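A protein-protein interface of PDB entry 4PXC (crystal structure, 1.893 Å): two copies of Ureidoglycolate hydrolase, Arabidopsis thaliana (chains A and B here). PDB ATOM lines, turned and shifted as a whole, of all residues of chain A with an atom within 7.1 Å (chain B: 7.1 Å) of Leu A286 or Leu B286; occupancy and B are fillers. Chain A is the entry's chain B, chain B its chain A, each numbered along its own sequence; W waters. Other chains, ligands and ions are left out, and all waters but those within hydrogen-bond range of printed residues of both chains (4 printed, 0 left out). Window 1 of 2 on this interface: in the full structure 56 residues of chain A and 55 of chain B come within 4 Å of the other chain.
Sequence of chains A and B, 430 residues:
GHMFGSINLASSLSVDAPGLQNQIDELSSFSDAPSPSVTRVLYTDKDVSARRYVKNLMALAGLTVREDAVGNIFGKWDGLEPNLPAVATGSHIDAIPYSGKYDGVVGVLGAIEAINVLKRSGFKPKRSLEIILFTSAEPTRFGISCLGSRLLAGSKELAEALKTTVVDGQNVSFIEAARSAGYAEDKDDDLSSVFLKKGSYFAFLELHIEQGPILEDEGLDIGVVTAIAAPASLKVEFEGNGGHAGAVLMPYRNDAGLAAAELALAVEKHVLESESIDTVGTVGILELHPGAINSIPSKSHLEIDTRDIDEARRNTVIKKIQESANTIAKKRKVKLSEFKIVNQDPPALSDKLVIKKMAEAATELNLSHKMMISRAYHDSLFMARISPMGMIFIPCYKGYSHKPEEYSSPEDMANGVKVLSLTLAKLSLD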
ATOM      1  N   ALA A 256     -16.907 -28.368  -7.833  1.00  0.00           N
ATOM      2  CA  ALA A 256     -17.283 -29.150  -6.657  1.00  0.00           C
ATOM      3  C   ALA A 256     -18.747 -28.946  -6.285  1.00  0.00           C
ATOM      4  O   ALA A 256     -19.354 -29.780  -5.599  1.00  0.00           O
ATOM      5  CB  ALA A 256     -16.387 -28.794  -5.477  1.00  0.00           C
ATOM      6  N   GLY A 257     -19.310 -27.814  -6.697  1.00  0.00           N
ATOM      7  CA  GLY A 257     -20.703 -27.534  -6.388  1.00  0.00           C
ATOM      8  C   GLY A 257     -21.625 -28.381  -7.238  1.00  0.00           C
ATOM      9  O   GLY A 257     -22.698 -28.799  -6.801  1.00  0.00           O
ATOM     10  N   ALA A 260     -21.709 -31.801  -5.800  1.00  0.00           N
ATOM     11  CA  ALA A 260     -22.665 -31.803  -4.686  1.00  0.00           C
ATOM     12  C   ALA A 260     -24.115 -31.881  -5.166  1.00  0.00           C
ATOM     13  O   ALA A 260     -24.919 -32.647  -4.623  1.00  0.00           O
ATOM     14  CB  ALA A 260     -22.465 -30.581  -3.794  1.00  0.00           C
ATOM     15  N   ALA A 261     -24.450 -31.082  -6.177  1.00  0.00           N
ATOM     16  CA  ALA A 261     -25.793 -31.082  -6.749  1.00  0.00           C
ATOM     17  C   ALA A 261     -26.159 -32.477  -7.229  1.00  0.00           C
ATOM     18  O   ALA A 261     -27.272 -32.953  -6.995  1.00  0.00           O
ATOM     19  CB  ALA A 261     -25.866 -30.089  -7.912  1.00  0.00           C
ATOM     20  N   GLU A 262     -25.221 -33.125  -7.916  1.00  0.00           N
ATOM     21  CA  GLU A 262     -25.431 -34.484  -8.404  1.00  0.00           C
ATOM     22  C   GLU A 262     -25.600 -35.499  -7.274  1.00  0.00           C
ATOM     23  O   GLU A 262     -26.457 -36.380  -7.354  1.00  0.00           O
ATOM     24  CB  GLU A 262     -24.300 -34.882  -9.373  1.00  0.00           C
ATOM     25  CG  GLU A 262     -24.390 -34.110 -10.702  1.00  0.00           C
ATOM     26  CD  GLU A 262     -23.186 -34.302 -11.616  1.00  0.00           C
ATOM     27  OE1 GLU A 262     -22.068 -34.522 -11.108  1.00  0.00           O
ATOM     28  OE2 GLU A 262     -23.364 -34.225 -12.851  1.00  0.00           O
ATOM     29  N   LEU A 263     -24.818 -35.366  -6.206  1.00  0.00           N
ATOM     30  CA  LEU A 263     -24.953 -36.300  -5.082  1.00  0.00           C
ATOM     31  C   LEU A 263     -26.300 -36.114  -4.376  1.00  0.00           C
ATOM     32  O   LEU A 263     -26.940 -37.092  -3.996  1.00  0.00           O
ATOM     33  CB  LEU A 263     -23.792 -36.167  -4.090  1.00  0.00           C
ATOM     34  CG  LEU A 263     -23.798 -37.189  -2.944  1.00  0.00           C
ATOM     35  CD1 LEU A 263     -23.869 -38.611  -3.498  1.00  0.00           C
ATOM     36  CD2 LEU A 263     -22.582 -37.039  -2.064  1.00  0.00           C
ATOM     37  N   ALA A 264     -26.741 -34.869  -4.218  1.00  0.00           N
ATOM     38  CA  ALA A 264     -28.020 -34.599  -3.561  1.00  0.00           C
ATOM     39  C   ALA A 264     -29.169 -35.277  -4.308  1.00  0.00           C
ATOM     40  O   ALA A 264     -30.064 -35.888  -3.689  1.00  0.00           O
ATOM     41  CB  ALA A 264     -28.260 -33.099  -3.457  1.00  0.00           C
ATOM     42  N   VAL A 283     -30.913 -33.996   1.992  1.00  0.00           N
ATOM     43  CA  VAL A 283     -29.718 -33.172   2.115  1.00  0.00           C
ATOM     44  C   VAL A 283     -30.130 -31.847   2.756  1.00  0.00           C
ATOM     45  O   VAL A 283     -30.629 -30.939   2.075  1.00  0.00           O
ATOM     46  CB  VAL A 283     -29.020 -32.953   0.757  1.00  0.00           C
ATOM     47  CG1 VAL A 283     -27.794 -32.070   0.932  1.00  0.00           C
ATOM     48  CG2 VAL A 283     -28.626 -34.292   0.164  1.00  0.00           C
ATOM     49  N   GLY A 284     -29.943 -31.748   4.070  1.00  0.00           N
ATOM     50  CA  GLY A 284     -30.353 -30.555   4.797  1.00  0.00           C
ATOM     51  C   GLY A 284     -29.283 -29.479   4.815  1.00  0.00           C
ATOM     52  O   GLY A 284     -29.564 -28.301   5.079  1.00  0.00           O
ATOM     53  N   ILE A 285     -28.049 -29.893   4.557  1.00  0.00           N
ATOM     54  CA  ILE A 285     -26.919 -28.983   4.532  1.00  0.00           C
ATOM     55  C   ILE A 285     -26.119 -29.203   3.254  1.00  0.00           C
ATOM     56  O   ILE A 285     -25.738 -30.336   2.935  1.00  0.00           O
ATOM     57  CB  ILE A 285     -25.998 -29.212   5.760  1.00  0.00           C
ATOM     58  CG1 ILE A 285     -26.689 -28.704   7.036  1.00  0.00           C
ATOM     59  CG2 ILE A 285     -24.630 -28.539   5.559  1.00  0.00           C
ATOM     60  CD1 ILE A 285     -25.904 -28.948   8.307  1.00  0.00           C
ATOM     61  N   LEU A 286     -25.900 -28.127   2.505  1.00  0.00           N
ATOM     62  CA  LEU A 286     -25.044 -28.172   1.320  1.00  0.00           C
ATOM     63  C   LEU A 286     -24.354 -26.816   1.259  1.00  0.00           C
ATOM     64  O   LEU A 286     -25.018 -25.814   0.999  1.00  0.00           O
ATOM     65  CB  LEU A 286     -25.883 -28.434   0.058  1.00  0.00           C
ATOM     66  CG  LEU A 286     -25.164 -28.852  -1.235  1.00  0.00           C
ATOM     67  CD1 LEU A 286     -26.154 -29.378  -2.273  1.00  0.00           C
ATOM     68  CD2 LEU A 286     -24.376 -27.695  -1.840  1.00  0.00           C
ATOM     69  N   GLU A 287     -23.039 -26.789   1.496  1.00  0.00           N
ATOM     70  CA  GLU A 287     -22.280 -25.540   1.550  1.00  0.00           C
ATOM     71  C   GLU A 287     -21.175 -25.492   0.503  1.00  0.00           C
ATOM     72  O   GLU A 287     -20.434 -26.454   0.334  1.00  0.00           O
ATOM     73  CB  GLU A 287     -21.621 -25.359   2.919  1.00  0.00           C
ATOM     74  CG  GLU A 287     -22.555 -25.367   4.116  1.00  0.00           C
ATOM     75  CD  GLU A 287     -21.784 -25.275   5.417  1.00  0.00           C
ATOM     76  OE1 GLU A 287     -20.544 -25.071   5.340  1.00  0.00           O
ATOM     77  OE2 GLU A 287     -22.401 -25.414   6.502  1.00  0.00           O
ATOM     78  N   LEU A 288     -21.043 -24.358  -0.175  1.00  0.00           N
ATOM     79  CA  LEU A 288     -19.954 -24.178  -1.128  1.00  0.00           C
ATOM     80  C   LEU A 288     -18.834 -23.285  -0.581  1.00  0.00           C
ATOM     81  O   LEU A 288     -19.090 -22.335   0.167  1.00  0.00           O
ATOM     82  CB  LEU A 288     -20.496 -23.596  -2.437  1.00  0.00           C
ATOM     83  CG  LEU A 288     -21.691 -24.344  -3.034  1.00  0.00           C
ATOM     84  CD1 LEU A 288     -22.160 -23.648  -4.317  1.00  0.00           C
ATOM     85  CD2 LEU A 288     -21.352 -25.806  -3.314  1.00  0.00           C
ATOM     86  N   GLY A 291     -17.674 -19.834  -1.875  1.00  0.00           N
ATOM     87  CA  GLY A 291     -19.018 -19.284  -1.766  1.00  0.00           C
ATOM     88  C   GLY A 291     -19.073 -17.830  -2.212  1.00  0.00           C
ATOM     89  O   GLY A 291     -19.606 -16.964  -1.513  1.00  0.00           O
ATOM     90  N   PRO A 297     -16.658 -23.077  -7.199  1.00  0.00           N
ATOM     91  CA  PRO A 297     -16.501 -23.792  -5.924  1.00  0.00           C
ATOM     92  C   PRO A 297     -15.386 -24.812  -5.983  1.00  0.00           C
ATOM     93  O   PRO A 297     -15.357 -25.666  -6.881  1.00  0.00           O
ATOM     94  CB  PRO A 297     -17.855 -24.492  -5.736  1.00  0.00           C
ATOM     95  CG  PRO A 297     -18.815 -23.609  -6.468  1.00  0.00           C
ATOM     96  CD  PRO A 297     -18.054 -23.108  -7.677  1.00  0.00           C
ATOM     97  N   SER A 300     -17.010 -28.500  -1.656  1.00  0.00           N
ATOM     98  CA  SER A 300     -18.426 -28.571  -1.314  1.00  0.00           C
ATOM     99  C   SER A 300     -18.615 -29.569  -0.187  1.00  0.00           C
ATOM    100  O   SER A 300     -17.837 -30.515  -0.036  1.00  0.00           O
ATOM    101  CB  SER A 300     -19.283 -28.912  -2.527  1.00  0.00           C
ATOM    102  OG  SER A 300     -19.012 -30.214  -3.018  1.00  0.00           O
ATOM    103  N   HIS A 301     -19.648 -29.341   0.613  1.00  0.00           N
ATOM    104  CA  HIS A 301     -19.831 -30.063   1.860  1.00  0.00           C
ATOM    105  C   HIS A 301     -21.324 -30.385   1.964  1.00  0.00           C
ATOM    106  O   HIS A 301     -22.160 -29.489   1.840  1.00  0.00           O
ATOM    107  CB  HIS A 301     -19.335 -29.157   3.002  1.00  0.00           C
ATOM    108  CG  HIS A 301     -19.681 -29.625   4.384  1.00  0.00           C
ATOM    109  ND1 HIS A 301     -18.823 -30.386   5.151  1.00  0.00           N
ATOM    110  CD2 HIS A 301     -20.766 -29.387   5.164  1.00  0.00           C
ATOM    111  CE1 HIS A 301     -19.376 -30.625   6.328  1.00  0.00           C
ATOM    112  NE2 HIS A 301     -20.556 -30.028   6.362  1.00  0.00           N
ATOM    113  N   LEU A 302     -21.653 -31.667   2.124  1.00  0.00           N
ATOM    114  CA  LEU A 302     -23.042 -32.098   2.252  1.00  0.00           C
ATOM    115  C   LEU A 302     -23.207 -32.848   3.562  1.00  0.00           C
ATOM    116  O   LEU A 302     -22.320 -33.603   3.964  1.00  0.00           O
ATOM    117  CB  LEU A 302     -23.459 -33.040   1.109  1.00  0.00           C
ATOM    118  CG  LEU A 302     -23.372 -32.637  -0.364  1.00  0.00           C
ATOM    119  CD1 LEU A 302     -21.964 -32.915  -0.928  1.00  0.00           C
ATOM    120  CD2 LEU A 302     -24.439 -33.375  -1.169  1.00  0.00           C
ATOM    121  N   GLU A 303     -24.339 -32.641   4.231  1.00  0.00           N
ATOM    122  CA  GLU A 303     -24.683 -33.460   5.387  1.00  0.00           C
ATOM    123  C   GLU A 303     -26.031 -34.099   5.106  1.00  0.00           C
ATOM    124  O   GLU A 303     -27.014 -33.416   4.821  1.00  0.00           O
ATOM    125  CB  GLU A 303     -24.653 -32.649   6.688  1.00  0.00           C
ATOM    126  CG  GLU A 303     -23.304 -31.976   6.919  1.00  0.00           C
ATOM    127  CD  GLU A 303     -23.112 -31.439   8.325  1.00  0.00           C
ATOM    128  OE1 GLU A 303     -23.832 -31.880   9.255  1.00  0.00           O
ATOM    129  OE2 GLU A 303     -22.223 -30.573   8.500  1.00  0.00           O
ATOM    130  N   ALA B 256     -36.635 -27.615  -1.588  1.00  0.00           N
ATOM    131  CA  ALA B 256     -36.086 -26.432  -2.258  1.00  0.00           C
ATOM    132  C   ALA B 256     -34.609 -26.612  -2.597  1.00  0.00           C
ATOM    133  O   ALA B 256     -34.087 -25.991  -3.532  1.00  0.00           O
ATOM    134  CB  ALA B 256     -36.282 -25.186  -1.386  1.00  0.00           C
ATOM    135  N   GLY B 257     -33.934 -27.449  -1.815  1.00  0.00           N
ATOM    136  CA  GLY B 257     -32.551 -27.787  -2.083  1.00  0.00           C
ATOM    137  C   GLY B 257     -32.415 -28.540  -3.392  1.00  0.00           C
ATOM    138  O   GLY B 257     -31.513 -28.264  -4.188  1.00  0.00           O
ATOM    139  N   LEU B 258     -33.320 -29.485  -3.632  1.00  0.00           N
ATOM    140  CA  LEU B 258     -33.262 -30.286  -4.853  1.00  0.00           C
ATOM    141  C   LEU B 258     -33.613 -29.442  -6.083  1.00  0.00           C
ATOM    142  O   LEU B 258     -33.024 -29.626  -7.155  1.00  0.00           O
ATOM    143  CB  LEU B 258     -34.154 -31.527  -4.733  1.00  0.00           C
ATOM    144  CG  LEU B 258     -33.686 -32.454  -3.610  1.00  0.00           C
ATOM    145  CD1 LEU B 258     -34.529 -33.729  -3.576  1.00  0.00           C
ATOM    146  CD2 LEU B 258     -32.188 -32.769  -3.748  1.00  0.00           C
ATOM    147  N   ALA B 260     -32.802 -26.345  -6.376  1.00  0.00           N
ATOM    148  CA  ALA B 260     -31.558 -25.619  -6.584  1.00  0.00           C
ATOM    149  C   ALA B 260     -30.505 -26.485  -7.274  1.00  0.00           C
ATOM    150  O   ALA B 260     -29.822 -26.026  -8.200  1.00  0.00           O
ATOM    151  CB  ALA B 260     -31.033 -25.100  -5.254  1.00  0.00           C
ATOM    152  N   ALA B 261     -30.357 -27.723  -6.801  1.00  0.00           N
ATOM    153  CA  ALA B 261     -29.442 -28.681  -7.410  1.00  0.00           C
ATOM    154  C   ALA B 261     -29.768 -28.827  -8.890  1.00  0.00           C
ATOM    155  O   ALA B 261     -28.880 -28.794  -9.741  1.00  0.00           O
ATOM    156  CB  ALA B 261     -29.544 -30.043  -6.710  1.00  0.00           C
ATOM    157  N   GLU B 262     -31.049 -28.987  -9.196  1.00  0.00           N
ATOM    158  CA  GLU B 262     -31.470 -29.147 -10.583  1.00  0.00           C
ATOM    159  C   GLU B 262     -31.203 -27.888 -11.420  1.00  0.00           C
ATOM    160  O   GLU B 262     -30.775 -27.977 -12.582  1.00  0.00           O
ATOM    161  CB  GLU B 262     -32.947 -29.581 -10.647  1.00  0.00           C
ATOM    162  CG  GLU B 262     -33.143 -31.016 -10.165  1.00  0.00           C
ATOM    163  CD  GLU B 262     -34.606 -31.396  -9.991  1.00  0.00           C
ATOM    164  OE1 GLU B 262     -35.416 -30.520  -9.617  1.00  0.00           O
ATOM    165  OE2 GLU B 262     -34.935 -32.579 -10.221  1.00  0.00           O
ATOM    166  N   ALA B 264     -28.801 -25.638 -10.859  1.00  0.00           N
ATOM    167  CA  ALA B 264     -27.353 -25.500 -11.036  1.00  0.00           C
ATOM    168  C   ALA B 264     -26.868 -26.360 -12.196  1.00  0.00           C
ATOM    169  O   ALA B 264     -25.997 -25.942 -12.971  1.00  0.00           O
ATOM    170  CB  ALA B 264     -26.610 -25.855  -9.746  1.00  0.00           C
ATOM    171  N   VAL B 283     -22.530 -21.511 -10.832  1.00  0.00           N
ATOM    172  CA  VAL B 283     -23.230 -21.271  -9.572  1.00  0.00           C
ATOM    173  C   VAL B 283     -22.177 -21.244  -8.463  1.00  0.00           C
ATOM    174  O   VAL B 283     -21.728 -22.295  -7.985  1.00  0.00           O
ATOM    175  CB  VAL B 283     -24.300 -22.336  -9.285  1.00  0.00           C
ATOM    176  CG1 VAL B 283     -24.968 -22.059  -7.944  1.00  0.00           C
ATOM    177  CG2 VAL B 283     -25.336 -22.352 -10.403  1.00  0.00           C
ATOM    178  N   GLY B 284     -21.756 -20.035  -8.088  1.00  0.00           N
ATOM    179  CA  GLY B 284     -20.745 -19.866  -7.056  1.00  0.00           C
ATOM    180  C   GLY B 284     -21.330 -19.812  -5.652  1.00  0.00           C
ATOM    181  O   GLY B 284     -20.627 -20.012  -4.652  1.00  0.00           O
ATOM    182  N   ILE B 285     -22.627 -19.539  -5.582  1.00  0.00           N
ATOM    183  CA  ILE B 285     -23.320 -19.440  -4.306  1.00  0.00           C
ATOM    184  C   ILE B 285     -24.567 -20.301  -4.372  1.00  0.00           C
ATOM    185  O   ILE B 285     -25.387 -20.147  -5.283  1.00  0.00           O
ATOM    186  CB  ILE B 285     -23.695 -17.976  -3.982  1.00  0.00           C
ATOM    187  CG1 ILE B 285     -22.435 -17.196  -3.575  1.00  0.00           C
ATOM    188  CG2 ILE B 285     -24.717 -17.916  -2.847  1.00  0.00           C
ATOM    189  CD1 ILE B 285     -22.649 -15.714  -3.339  1.00  0.00           C
ATOM    190  N   LEU B 286     -24.680 -21.239  -3.434  1.00  0.00           N
ATOM    191  CA  LEU B 286     -25.888 -22.036  -3.283  1.00  0.00           C
ATOM    192  C   LEU B 286     -26.083 -22.241  -1.793  1.00  0.00           C
ATOM    193  O   LEU B 286     -25.313 -22.974  -1.159  1.00  0.00           O
ATOM    194  CB  LEU B 286     -25.760 -23.384  -4.019  1.00  0.00           C
ATOM    195  CG  LEU B 286     -27.044 -24.190  -4.312  1.00  0.00           C
ATOM    196  CD1 LEU B 286     -26.758 -25.372  -5.230  1.00  0.00           C
ATOM    197  CD2 LEU B 286     -27.734 -24.690  -3.037  1.00  0.00           C
ATOM    198  N   GLU B 287     -27.092 -21.585  -1.225  1.00  0.00           N
ATOM    199  CA  GLU B 287     -27.325 -21.700   0.215  1.00  0.00           C
ATOM    200  C   GLU B 287     -28.692 -22.300   0.528  1.00  0.00           C
ATOM    201  O   GLU B 287     -29.679 -21.994  -0.153  1.00  0.00           O
ATOM    202  CB  GLU B 287     -27.143 -20.359   0.938  1.00  0.00           C
ATOM    203  CG  GLU B 287     -27.900 -19.195   0.338  1.00  0.00           C
ATOM    204  CD  GLU B 287     -28.387 -18.190   1.383  1.00  0.00           C
ATOM    205  OE1 GLU B 287     -29.601 -17.886   1.392  1.00  0.00           O
ATOM    206  OE2 GLU B 287     -27.552 -17.709   2.186  1.00  0.00           O
ATOM    207  N   LEU B 288     -28.733 -23.166   1.543  1.00  0.00           N
ATOM    208  CA  LEU B 288     -29.988 -23.772   1.997  1.00  0.00           C
ATOM    209  C   LEU B 288     -30.444 -23.154   3.328  1.00  0.00           C
ATOM    210  O   LEU B 288     -29.617 -22.865   4.204  1.00  0.00           O
ATOM    211  CB  LEU B 288     -29.836 -25.289   2.156  1.00  0.00           C
ATOM    212  CG  LEU B 288     -29.305 -26.091   0.958  1.00  0.00           C
ATOM    213  CD1 LEU B 288     -29.307 -27.599   1.237  1.00  0.00           C
ATOM    214  CD2 LEU B 288     -30.119 -25.782  -0.299  1.00  0.00           C
ATOM    215  N   GLY B 291     -30.905 -24.878   6.785  1.00  0.00           N
ATOM    216  CA  GLY B 291     -29.539 -25.389   6.772  1.00  0.00           C
ATOM    217  C   GLY B 291     -29.216 -26.220   8.001  1.00  0.00           C
ATOM    218  O   GLY B 291     -28.195 -26.011   8.662  1.00  0.00           O
ATOM    219  N   PRO B 297     -34.873 -28.382   3.472  1.00  0.00           N
ATOM    220  CA  PRO B 297     -34.751 -26.969   3.091  1.00  0.00           C
ATOM    221  C   PRO B 297     -36.077 -26.390   2.609  1.00  0.00           C
ATOM    222  O   PRO B 297     -36.679 -26.952   1.695  1.00  0.00           O
ATOM    223  CB  PRO B 297     -33.760 -27.007   1.918  1.00  0.00           C
ATOM    224  CG  PRO B 297     -32.919 -28.228   2.181  1.00  0.00           C
ATOM    225  CD  PRO B 297     -33.888 -29.234   2.780  1.00  0.00           C
ATOM    226  N   SER B 300     -34.061 -22.084  -0.859  1.00  0.00           N
ATOM    227  CA  SER B 300     -32.728 -22.215  -1.413  1.00  0.00           C
ATOM    228  C   SER B 300     -32.455 -20.969  -2.225  1.00  0.00           C
ATOM    229  O   SER B 300     -33.371 -20.351  -2.779  1.00  0.00           O
ATOM    230  CB  SER B 300     -32.609 -23.475  -2.264  1.00  0.00           C
ATOM    231  OG  SER B 300     -33.482 -23.420  -3.379  1.00  0.00           O
ATOM    232  N   HIS B 301     -31.188 -20.596  -2.287  1.00  0.00           N
ATOM    233  CA  HIS B 301     -30.787 -19.322  -2.858  1.00  0.00           C
ATOM    234  C   HIS B 301     -29.573 -19.611  -3.733  1.00  0.00           C
ATOM    235  O   HIS B 301     -28.636 -20.283  -3.293  1.00  0.00           O
ATOM    236  CB  HIS B 301     -30.500 -18.352  -1.699  1.00  0.00           C
ATOM    237  CG  HIS B 301     -29.753 -17.109  -2.081  1.00  0.00           C
ATOM    238  ND1 HIS B 301     -30.387 -15.929  -2.409  1.00  0.00           N
ATOM    239  CD2 HIS B 301     -28.426 -16.851  -2.141  1.00  0.00           C
ATOM    240  CE1 HIS B 301     -29.481 -15.003  -2.679  1.00  0.00           C
ATOM    241  NE2 HIS B 301     -28.282 -15.537  -2.520  1.00  0.00           N
ATOM    242  N   LEU B 302     -29.638 -19.197  -4.996  1.00  0.00           N
ATOM    243  CA  LEU B 302     -28.536 -19.402  -5.932  1.00  0.00           C
ATOM    244  C   LEU B 302     -28.121 -18.052  -6.491  1.00  0.00           C
ATOM    245  O   LEU B 302     -28.966 -17.200  -6.776  1.00  0.00           O
ATOM    246  CB  LEU B 302     -28.936 -20.307  -7.117  1.00  0.00           C
ATOM    247  CG  LEU B 302     -29.467 -21.726  -6.932  1.00  0.00           C
ATOM    248  CD1 LEU B 302     -30.988 -21.717  -6.789  1.00  0.00           C
ATOM    249  CD2 LEU B 302     -29.048 -22.613  -8.109  1.00  0.00           C
ATOM    250  N   GLU B 303     -26.818 -17.851  -6.638  1.00  0.00           N
ATOM    251  CA  GLU B 303     -26.327 -16.693  -7.355  1.00  0.00           C
ATOM    252  C   GLU B 303     -25.504 -17.205  -8.520  1.00  0.00           C
ATOM    253  O   GLU B 303     -24.553 -17.976  -8.340  1.00  0.00           O
ATOM    254  CB  GLU B 303     -25.543 -15.769  -6.429  1.00  0.00           C
ATOM    255  CG  GLU B 303     -26.375 -15.371  -5.217  1.00  0.00           C
ATOM    256  CD  GLU B 303     -25.872 -14.134  -4.515  1.00  0.00           C
ATOM    257  OE1 GLU B 303     -25.084 -13.373  -5.123  1.00  0.00           O
ATOM    258  OE2 GLU B 303     -26.282 -13.925  -3.348  1.00  0.00           O
HETATM  259  O   HOH W   1     -32.018 -27.388   5.807  1.00  0.00           O
HETATM  260  O   HOH W   2     -17.959 -20.353  -4.772  1.00  0.00           O
HETATM  261  O   HOH W   3     -26.049 -23.695   2.519  1.00  0.00           O
HETATM  262  O   HOH W   4     -23.165 -22.548   0.515  1.00  0.00           O
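The backbone carbonyl oxygen of Pro A297 is in hydrogen-bond range of the backbone NH of Ala A256 (3.3 Å). The backbone carbonyl oxygen of Ile A285 sits at hydrogen-bond distance from the backbone NH of Glu A303 (3.0 Å). The backbone NH (N) of Gly B284 lies within hydrogen-bond range of the backbone carbonyl oxygen (O) of Glu B303 (3.5 Å). O of Glu A303 is in hydrogen-bond range of N of Gly A284, at 3.5 Å. The backbone NH (N) of Ala B256 sits at hydrogen-bond distance from the backbone carbonyl oxygen (O) of Pro B297, 3.3 Å away. The backbone carbonyl oxygen of Ile B285 lies within hydrogen-bond range of the backbone NH of Glu B303, at 3.0 Å.
Among the printed residues, merely in contact across the chains: Gly A284 with Gly B291, Gly A291 with Gly B284, Ile A285 with Gly B291, Gly A291 with Ile B285, Pro A297 with Val B283, Val A283 with Pro B297, Leu A286 with Leu B286, Leu A288 with Leu B286, Leu A286 with Leu B288, Val A283 with Leu B288, Ala A261 with Ala B261, Ala A264 with Leu B258, Gly A284 with Leu B288, Leu A288 with Val B283 and Leu A288 with Gly B284.
Of the printed residues of chain B, Ala A261 touches Ala B261 (3.7 Å). Leu A286 touches two residues of chain B. His A301 touches none of the printed residues of chain B. Leu A302 touches none of the printed residues of chain B. Of the printed residues of chain A, Val B283 touches Leu A288 and Pro A297. Printed residues of chain A within 4 Å of Gly B284: Leu A288 (3.96 Å) and Gly A291 (3.4 Å). Of chain A, only Leu A286 and Leu A288 come within 4 Å of Leu B286. The nearest residue of chain B that does not touch Leu A286 is Glu B287 (4.8 Å). The nearest printed residue of chain A that does not touch Leu B288 is Ile A285 (4.1 Å).
Printed residues of chain B that touch a printed residue of chain A: Leu B258, Ala B261, Val B283, Gly B284, Ile B285, Leu B286, Leu B288, Gly B291 and Pro B297. Hydrophobic or aromatic side chains of chain B that line the printed part of chain A: Leu B258, Ala B261, Ile B285, Leu B286, Leu B288 and Pro B297. Of the 19 printed residues of chain A, 9 touch a printed residue of chain B. Printed residues of chain A that touch a printed residue of chain B: Ala A261, Ala A264, Val A283, Gly A284, Ile A285, Leu A286, Leu A288, Gly A291 and Pro A297. Hydrophobic or aromatic side chains of chain A within 4 Å of the printed part of chain B: Ala A261, Ala A264, Ile A285, Leu A286, Leu A288 and Pro A297. Among the printed residues, 15 pairs touch across the chains.
Ala B261 touches its own counterpart, Ala A261. Val A283 touches Pro B297, and with the chains exchanged Pro A297 touches Val B283. Gly A284 touches Leu B288, and with the chains exchanged Leu A288 touches Gly B284. Leu A286 touches Leu B288, and with the chains exchanged Leu A288 touches Leu B286. 18 positions are printed for both chains. Of the 15 pairs that touch across the chains among the printed residues, 14 have their exchanged pair printed and touching as well.
Water W2 lies within hydrogen-bond range of O of Gly B284 (2.7 Å) and N of Gly A291 (3.0 Å). Water W1 lies within hydrogen-bond range of O of Gly A284 (2.7 Å) and N of Gly B291 (2.9 Å). Water W4 lies within hydrogen-bond range of O of Leu B286 (2.8 Å) and N of Leu A288 (2.9 Å). Water W3 bridges O of Leu A286 (2.8 Å) and N of Leu B288 (2.9 Å).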
